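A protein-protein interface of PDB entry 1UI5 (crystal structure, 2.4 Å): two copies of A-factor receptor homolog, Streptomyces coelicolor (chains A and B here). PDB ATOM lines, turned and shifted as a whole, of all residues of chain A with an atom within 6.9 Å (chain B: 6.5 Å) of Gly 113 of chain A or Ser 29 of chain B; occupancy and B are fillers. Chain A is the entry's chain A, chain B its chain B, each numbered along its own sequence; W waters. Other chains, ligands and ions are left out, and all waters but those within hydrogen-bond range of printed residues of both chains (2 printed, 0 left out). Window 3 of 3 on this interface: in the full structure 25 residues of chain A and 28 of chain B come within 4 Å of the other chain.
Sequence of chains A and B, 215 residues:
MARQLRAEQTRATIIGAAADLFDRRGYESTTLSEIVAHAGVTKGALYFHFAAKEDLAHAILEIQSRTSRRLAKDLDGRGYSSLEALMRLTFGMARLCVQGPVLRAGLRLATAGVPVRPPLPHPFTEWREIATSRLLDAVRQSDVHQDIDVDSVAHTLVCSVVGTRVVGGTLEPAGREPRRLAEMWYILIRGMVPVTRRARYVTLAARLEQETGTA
Glu 28 of chain B touches its own counterpart, Glu 28 of chain A.
Positions printed for both chains: 28 and 108.
Of the 9 pairs that touch across the chains among the printed residues, 1 has its exchanged pair printed and touching as well.
Water W1 bridges the backbone carbonyl oxygen of Thr 111 of chain A (2.6 Å) and the guanidinium group of Arg 108 of chain B (2.6 Å).
Water W2 lies within hydrogen-bond range of the backbone carbonyl oxygen (O) of Thr 111 of chain A (3.2 Å), the backbone carbonyl oxygen (O) of Arg 108 of chain B (3.3 Å) and the backbone NH (N) of Tyr 27 of chain B (3.5 Å).
Printed residues of chain B that touch a printed residue of chain A: Arg 25, Glu 28, Ser 29, Arg 108 and Val 167.
Hydrophobic or aromatic side chains of chain B within 4 Å of the printed part of chain A: Val 167.
Of the 11 printed residues of chain A, 6 touch a printed residue of chain B.
Hydrophobic or aromatic side chains of chain A within 4 Å of the printed part of chain B: His 122.
Among the printed residues, 9 pairs touch across the chains.
The side-chain hydroxyl (OG1) of Thr 111 of chain A lies within hydrogen-bond range of the backbone carbonyl oxygen (O) of Arg 108 of chain A, at 2.8 Å.
The backbone carbonyl oxygen of Arg 25 of chain B lies within hydrogen-bond range of the side-chain hydroxyl of Ser 29 of chain B, at 3.3 Å.
The backbone carbonyl oxygen (O) of Glu 28 of chain B lies within hydrogen-bond range of the side-chain amino group (NZ) of Lys 53 of chain B (3.0 Å).
NH2 of Arg 108 of chain B lies within hydrogen-bond range of O of Thr 111 of chain A (2.9 Å).
The side-chain carboxylate (OE1) of Glu 28 of chain A lies close to the side-chain carboxylate (OE1) of Glu 28 of chain B.
Of the printed residues of chain B, Gly 113 of chain A touches Arg 25 (3.6 Å), Ser 29 (3.9 Å) and Arg 108 (3.8 Å).
Ser 29 of chain B touches one residue of chain A.
Printed residues of chain A within 4 Å of Arg 108 of chain B: Thr 111 (2.9 Å) and Gly 113 (3.8 Å).
Of the printed residues of chain A, Arg 25 of chain B touches Ala 112 and Gly 113.
Printed residues of chain B within 4 Å of His 122 of chain A: Val 167 (3.7 Å).
Of the printed residues of chain A, Glu 28 of chain B touches Glu 28.
Of the printed residues of chain A, Val 167 of chain B touches Ala 110, Thr 111 and His 122.
Pro 115 of chain A touches none of the printed residues of chain B.
Gly 26 of chain B touches none of the printed residues of chain A.
The nearest residue of chain B that does not touch Gly 113 of chain A is Gly 26 of chain B (4.8 Å).
The nearest residue of chain A that does not touch Ser 29 of chain B is Ala 112 of chain A (4.3 Å).
O of Ala 110 of chain A touches CB of Val 167 of chain B, at 3.7 Å.
Val 167 of chain B touches Thr 111 of chain A (CG1 to CA, 3.8 Å).
Ala 112 of chain A touches Arg 25 of chain B (O to O, 3.99 Å).
O of Arg 25 of chain B touches O of Gly 113 of chain A, at 3.6 Å.
Gly 113 of chain A touches Ser 29 of chain B (O to OG, 3.9 Å).
Arg 108 of chain B touches Gly 113 of chain A (NH2 to N, 3.8 Å).
CG2 of Val 167 of chain B touches CE1 of His 122 of chain A, 3.7 Å away.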
ATOM      1  N   GLU A  28       1.744  29.087 -30.425  1.00  0.00           N
ATOM      2  CA  GLU A  28       2.743  28.102 -30.810  1.00  0.00           C
ATOM      3  C   GLU A  28       3.525  28.462 -32.065  1.00  0.00           C
ATOM      4  O   GLU A  28       4.738  28.324 -32.075  1.00  0.00           O
ATOM      5  CB  GLU A  28       2.135  26.686 -30.976  1.00  0.00           C
ATOM      6  CG  GLU A  28       3.214  25.614 -31.021  1.00  0.00           C
ATOM      7  CD  GLU A  28       2.721  24.206 -31.344  1.00  0.00           C
ATOM      8  OE1 GLU A  28       1.525  24.024 -31.670  1.00  0.00           O
ATOM      9  OE2 GLU A  28       3.556  23.268 -31.290  1.00  0.00           O
ATOM     10  N   ARG A 108      -6.867  34.203 -26.226  1.00  0.00           N
ATOM     11  CA  ARG A 108      -6.355  33.134 -27.077  1.00  0.00           C
ATOM     12  C   ARG A 108      -5.297  32.309 -26.365  1.00  0.00           C
ATOM     13  O   ARG A 108      -5.147  31.107 -26.624  1.00  0.00           O
ATOM     14  CB  ARG A 108      -5.773  33.683 -28.385  1.00  0.00           C
ATOM     15  CG  ARG A 108      -6.766  33.780 -29.559  1.00  0.00           C
ATOM     16  CD  ARG A 108      -8.125  34.360 -29.172  1.00  0.00           C
ATOM     17  NE  ARG A 108      -8.685  35.244 -30.187  1.00  0.00           N
ATOM     18  CZ  ARG A 108      -9.611  36.187 -29.946  1.00  0.00           C
ATOM     19  NH1 ARG A 108     -10.098  36.373 -28.707  1.00  0.00           N
ATOM     20  NH2 ARG A 108     -10.071  36.949 -30.958  1.00  0.00           N
ATOM     21  N   LEU A 109      -4.528  32.935 -25.483  1.00  0.00           N
ATOM     22  CA  LEU A 109      -3.527  32.198 -24.748  1.00  0.00           C
ATOM     23  C   LEU A 109      -4.211  31.223 -23.777  1.00  0.00           C
ATOM     24  O   LEU A 109      -3.742  30.111 -23.579  1.00  0.00           O
ATOM     25  CB  LEU A 109      -2.602  33.154 -24.002  1.00  0.00           C
ATOM     26  CG  LEU A 109      -1.716  34.044 -24.868  1.00  0.00           C
ATOM     27  CD1 LEU A 109      -1.128  35.174 -24.043  1.00  0.00           C
ATOM     28  CD2 LEU A 109      -0.623  33.243 -25.529  1.00  0.00           C
ATOM     29  N   ALA A 110      -5.317  31.667 -23.175  1.00  0.00           N
ATOM     30  CA  ALA A 110      -6.086  30.828 -22.259  1.00  0.00           C
ATOM     31  C   ALA A 110      -6.713  29.649 -22.963  1.00  0.00           C
ATOM     32  O   ALA A 110      -6.635  28.538 -22.463  1.00  0.00           O
ATOM     33  CB  ALA A 110      -7.162  31.630 -21.575  1.00  0.00           C
ATOM     34  N   THR A 111      -7.298  29.869 -24.136  1.00  0.00           N
ATOM     35  CA  THR A 111      -7.940  28.773 -24.878  1.00  0.00           C
ATOM     36  C   THR A 111      -6.951  27.715 -25.293  1.00  0.00           C
ATOM     37  O   THR A 111      -7.291  26.534 -25.326  1.00  0.00           O
ATOM     38  CB  THR A 111      -8.612  29.261 -26.154  1.00  0.00           C
ATOM     39  OG1 THR A 111      -7.594  29.731 -27.054  1.00  0.00           O
ATOM     40  CG2 THR A 111      -9.546  30.454 -25.893  1.00  0.00           C
ATOM     41  N   ALA A 112      -5.728  28.130 -25.610  1.00  0.00           N
ATOM     42  CA  ALA A 112      -4.687  27.210 -26.056  1.00  0.00           C
ATOM     43  C   ALA A 112      -3.911  26.577 -24.894  1.00  0.00           C
ATOM     44  O   ALA A 112      -3.031  25.748 -25.093  1.00  0.00           O
ATOM     45  CB  ALA A 112      -3.739  27.932 -27.023  1.00  0.00           C
ATOM     46  N   GLY A 113      -4.194  27.003 -23.677  1.00  0.00           N
ATOM     47  CA  GLY A 113      -3.627  26.340 -22.512  1.00  0.00           C
ATOM     48  C   GLY A 113      -2.191  26.667 -22.119  1.00  0.00           C
ATOM     49  O   GLY A 113      -1.537  25.890 -21.409  1.00  0.00           O
ATOM     50  N   VAL A 114      -1.700  27.821 -22.561  1.00  0.00           N
ATOM     51  CA  VAL A 114      -0.388  28.312 -22.137  1.00  0.00           C
ATOM     52  C   VAL A 114      -0.446  28.562 -20.639  1.00  0.00           C
ATOM     53  O   VAL A 114      -1.274  29.315 -20.168  1.00  0.00           O
ATOM     54  CB  VAL A 114      -0.041  29.619 -22.855  1.00  0.00           C
ATOM     55  CG1 VAL A 114       1.161  30.278 -22.217  1.00  0.00           C
ATOM     56  CG2 VAL A 114       0.197  29.355 -24.353  1.00  0.00           C
ATOM     57  N   PRO A 115       0.428  27.951 -19.870  1.00  0.00           N
ATOM     58  CA  PRO A 115       0.310  28.036 -18.404  1.00  0.00           C
ATOM     59  C   PRO A 115       0.343  29.457 -17.875  1.00  0.00           C
ATOM     60  O   PRO A 115       1.039  30.312 -18.422  1.00  0.00           O
ATOM     61  CB  PRO A 115       1.516  27.252 -17.891  1.00  0.00           C
ATOM     62  CG  PRO A 115       1.933  26.381 -19.061  1.00  0.00           C
ATOM     63  CD  PRO A 115       1.588  27.165 -20.305  1.00  0.00           C
ATOM     64  N   VAL A 116      -0.451  29.703 -16.841  1.00  0.00           N
ATOM     65  CA  VAL A 116      -0.442  30.967 -16.145  1.00  0.00           C
ATOM     66  C   VAL A 116       0.556  30.806 -15.007  1.00  0.00           C
ATOM     67  O   VAL A 116       0.597  29.764 -14.371  1.00  0.00           O
ATOM     68  CB  VAL A 116      -1.829  31.321 -15.575  1.00  0.00           C
ATOM     69  CG1 VAL A 116      -1.858  32.766 -15.115  1.00  0.00           C
ATOM     70  CG2 VAL A 116      -2.925  31.070 -16.607  1.00  0.00           C
ATOM     71  N   HIS A 122      -5.766  31.599 -12.982  1.00  0.00           N
ATOM     72  CA  HIS A 122      -6.328  31.466 -14.311  1.00  0.00           C
ATOM     73  C   HIS A 122      -7.384  32.576 -14.506  1.00  0.00           C
ATOM     74  O   HIS A 122      -8.213  32.798 -13.639  1.00  0.00           O
ATOM     75  CB  HIS A 122      -6.955  30.083 -14.510  1.00  0.00           C
ATOM     76  CG  HIS A 122      -7.114  29.715 -15.953  1.00  0.00           C
ATOM     77  ND1 HIS A 122      -8.029  30.327 -16.783  1.00  0.00           N
ATOM     78  CD2 HIS A 122      -6.419  28.850 -16.730  1.00  0.00           C
ATOM     79  CE1 HIS A 122      -7.922  29.820 -17.997  1.00  0.00           C
ATOM     80  NE2 HIS A 122      -6.941  28.933 -17.994  1.00  0.00           N
ATOM     81  N   ARG B  25      -4.599  20.143 -20.765  1.00  0.00           N
ATOM     82  CA  ARG B  25      -3.451  20.977 -21.037  1.00  0.00           C
ATOM     83  C   ARG B  25      -3.523  21.737 -22.368  1.00  0.00           C
ATOM     84  O   ARG B  25      -2.700  22.651 -22.596  1.00  0.00           O
ATOM     85  CB  ARG B  25      -2.179  20.108 -21.005  1.00  0.00           C
ATOM     86  CG  ARG B  25      -1.814  19.596 -19.615  1.00  0.00           C
ATOM     87  CD  ARG B  25      -0.437  18.913 -19.513  1.00  0.00           C
ATOM     88  NE  ARG B  25      -0.294  18.106 -18.295  1.00  0.00           N
ATOM     89  CZ  ARG B  25       0.484  17.026 -18.189  1.00  0.00           C
ATOM     90  NH1 ARG B  25       1.214  16.591 -19.227  1.00  0.00           N
ATOM     91  NH2 ARG B  25       0.543  16.373 -17.022  1.00  0.00           N
ATOM     92  N   GLY B  26      -4.504  21.414 -23.216  1.00  0.00           N
ATOM     93  CA  GLY B  26      -4.619  22.045 -24.522  1.00  0.00           C
ATOM     94  C   GLY B  26      -3.944  21.198 -25.603  1.00  0.00           C
ATOM     95  O   GLY B  26      -3.128  20.317 -25.312  1.00  0.00           O
ATOM     96  N   TYR B  27      -4.292  21.468 -26.856  1.00  0.00           N
ATOM     97  CA  TYR B  27      -3.724  20.785 -28.001  1.00  0.00           C
ATOM     98  C   TYR B  27      -2.287  21.180 -28.265  1.00  0.00           C
ATOM     99  O   TYR B  27      -1.450  20.319 -28.392  1.00  0.00           O
ATOM    100  CB  TYR B  27      -4.548  21.069 -29.263  1.00  0.00           C
ATOM    101  CG  TYR B  27      -4.080  20.337 -30.526  1.00  0.00           C
ATOM    102  CD1 TYR B  27      -4.170  18.953 -30.629  1.00  0.00           C
ATOM    103  CD2 TYR B  27      -3.567  21.043 -31.616  1.00  0.00           C
ATOM    104  CE1 TYR B  27      -3.778  18.284 -31.775  1.00  0.00           C
ATOM    105  CE2 TYR B  27      -3.156  20.385 -32.775  1.00  0.00           C
ATOM    106  CZ  TYR B  27      -3.270  18.992 -32.841  1.00  0.00           C
ATOM    107  OH  TYR B  27      -2.868  18.307 -33.965  1.00  0.00           O
ATOM    108  N   GLU B  28      -2.008  22.480 -28.264  1.00  0.00           N
ATOM    109  CA  GLU B  28      -0.730  23.013 -28.734  1.00  0.00           C
ATOM    110  C   GLU B  28       0.468  22.641 -27.892  1.00  0.00           C
ATOM    111  O   GLU B  28       1.499  22.249 -28.422  1.00  0.00           O
ATOM    112  CB  GLU B  28      -0.790  24.533 -28.889  1.00  0.00           C
ATOM    113  CG  GLU B  28      -1.911  25.037 -29.785  1.00  0.00           C
ATOM    114  CD  GLU B  28      -1.645  24.863 -31.276  1.00  0.00           C
ATOM    115  OE1 GLU B  28      -1.042  25.767 -31.911  1.00  0.00           O
ATOM    116  OE2 GLU B  28      -2.094  23.833 -31.830  1.00  0.00           O
ATOM    117  N   SER B  29       0.352  22.764 -26.586  1.00  0.00           N
ATOM    118  CA  SER B  29       1.498  22.466 -25.720  1.00  0.00           C
ATOM    119  C   SER B  29       1.620  20.965 -25.344  1.00  0.00           C
ATOM    120  O   SER B  29       2.568  20.574 -24.642  1.00  0.00           O
ATOM    121  CB  SER B  29       1.485  23.365 -24.475  1.00  0.00           C
ATOM    122  OG  SER B  29       0.238  23.334 -23.811  1.00  0.00           O
ATOM    123  N   THR B  30       0.682  20.137 -25.812  1.00  0.00           N
ATOM    124  CA  THR B  30       0.754  18.707 -25.564  1.00  0.00           C
ATOM    125  C   THR B  30       1.584  18.018 -26.672  1.00  0.00           C
ATOM    126  O   THR B  30       1.288  18.130 -27.864  1.00  0.00           O
ATOM    127  CB  THR B  30      -0.665  18.105 -25.475  1.00  0.00           C
ATOM    128  OG1 THR B  30      -1.336  18.567 -24.300  1.00  0.00           O
ATOM    129  CG2 THR B  30      -0.619  16.621 -25.248  1.00  0.00           C
ATOM    130  N   THR B  31       2.635  17.311 -26.274  1.00  0.00           N
ATOM    131  CA  THR B  31       3.510  16.663 -27.243  1.00  0.00           C
ATOM    132  C   THR B  31       3.138  15.222 -27.446  1.00  0.00           C
ATOM    133  O   THR B  31       2.344  14.631 -26.705  1.00  0.00           O
ATOM    134  CB  THR B  31       4.981  16.735 -26.808  1.00  0.00           C
ATOM    135  OG1 THR B  31       5.178  15.922 -25.651  1.00  0.00           O
ATOM    136  CG2 THR B  31       5.357  18.161 -26.356  1.00  0.00           C
ATOM    137  N   GLU B  34       4.478  13.079 -24.528  1.00  0.00           N
ATOM    138  CA  GLU B  34       3.675  13.087 -23.321  1.00  0.00           C
ATOM    139  C   GLU B  34       2.538  12.093 -23.455  1.00  0.00           C
ATOM    140  O   GLU B  34       2.170  11.405 -22.496  1.00  0.00           O
ATOM    141  CB  GLU B  34       3.130  14.484 -23.035  1.00  0.00           C
ATOM    142  CG  GLU B  34       4.185  15.455 -22.489  1.00  0.00           C
ATOM    143  CD  GLU B  34       3.705  16.909 -22.418  1.00  0.00           C
ATOM    144  OE1 GLU B  34       2.725  17.262 -23.096  1.00  0.00           O
ATOM    145  OE2 GLU B  34       4.340  17.724 -21.707  1.00  0.00           O
ATOM    146  N   LYS B  53       0.147  14.653 -34.803  1.00  0.00           N
ATOM    147  CA  LYS B  53      -0.811  15.141 -33.837  1.00  0.00           C
ATOM    148  C   LYS B  53      -2.188  15.314 -34.465  1.00  0.00           C
ATOM    149  O   LYS B  53      -3.210  14.906 -33.911  1.00  0.00           O
ATOM    150  CB  LYS B  53      -0.340  16.491 -33.259  1.00  0.00           C
ATOM    151  CG  LYS B  53       0.071  16.430 -31.792  1.00  0.00           C
ATOM    152  CD  LYS B  53       0.891  17.672 -31.341  1.00  0.00           C
ATOM    153  CE  LYS B  53       0.012  18.634 -30.547  1.00  0.00           C
ATOM    154  NZ  LYS B  53       0.740  19.709 -29.868  1.00  0.00           N
ATOM    155  N   ARG B 108     -11.484  21.900 -27.688  1.00  0.00           N
ATOM    156  CA  ARG B 108     -10.095  22.347 -27.695  1.00  0.00           C
ATOM    157  C   ARG B 108      -9.515  22.258 -29.101  1.00  0.00           C
ATOM    158  O   ARG B 108      -8.773  23.123 -29.503  1.00  0.00           O
ATOM    159  CB  ARG B 108      -9.224  21.527 -26.736  1.00  0.00           C
ATOM    160  CG  ARG B 108      -9.781  21.351 -25.318  1.00  0.00           C
ATOM    161  CD  ARG B 108     -10.003  22.627 -24.576  1.00  0.00           C
ATOM    162  NE  ARG B 108      -8.788  23.439 -24.470  1.00  0.00           N
ATOM    163  CZ  ARG B 108      -7.930  23.438 -23.455  1.00  0.00           C
ATOM    164  NH1 ARG B 108      -8.081  22.626 -22.422  1.00  0.00           N
ATOM    165  NH2 ARG B 108      -6.896  24.285 -23.466  1.00  0.00           N
ATOM    166  N   VAL B 167     -11.788  25.663 -21.345  1.00  0.00           N
ATOM    167  CA  VAL B 167     -10.385  25.867 -21.650  1.00  0.00           C
ATOM    168  C   VAL B 167      -9.435  25.168 -20.654  1.00  0.00           C
ATOM    169  O   VAL B 167      -8.311  25.630 -20.410  1.00  0.00           O
ATOM    170  CB  VAL B 167     -10.027  27.383 -21.685  1.00  0.00           C
ATOM    171  CG1 VAL B 167     -10.914  28.100 -22.666  1.00  0.00           C
ATOM    172  CG2 VAL B 167     -10.087  27.993 -20.318  1.00  0.00           C
HETATM  173  O   HOH W   1      -9.690  25.678 -25.514  1.00  0.00           O
HETATM  174  O   HOH W   2      -6.631  23.998 -27.101  1.00  0.00           O
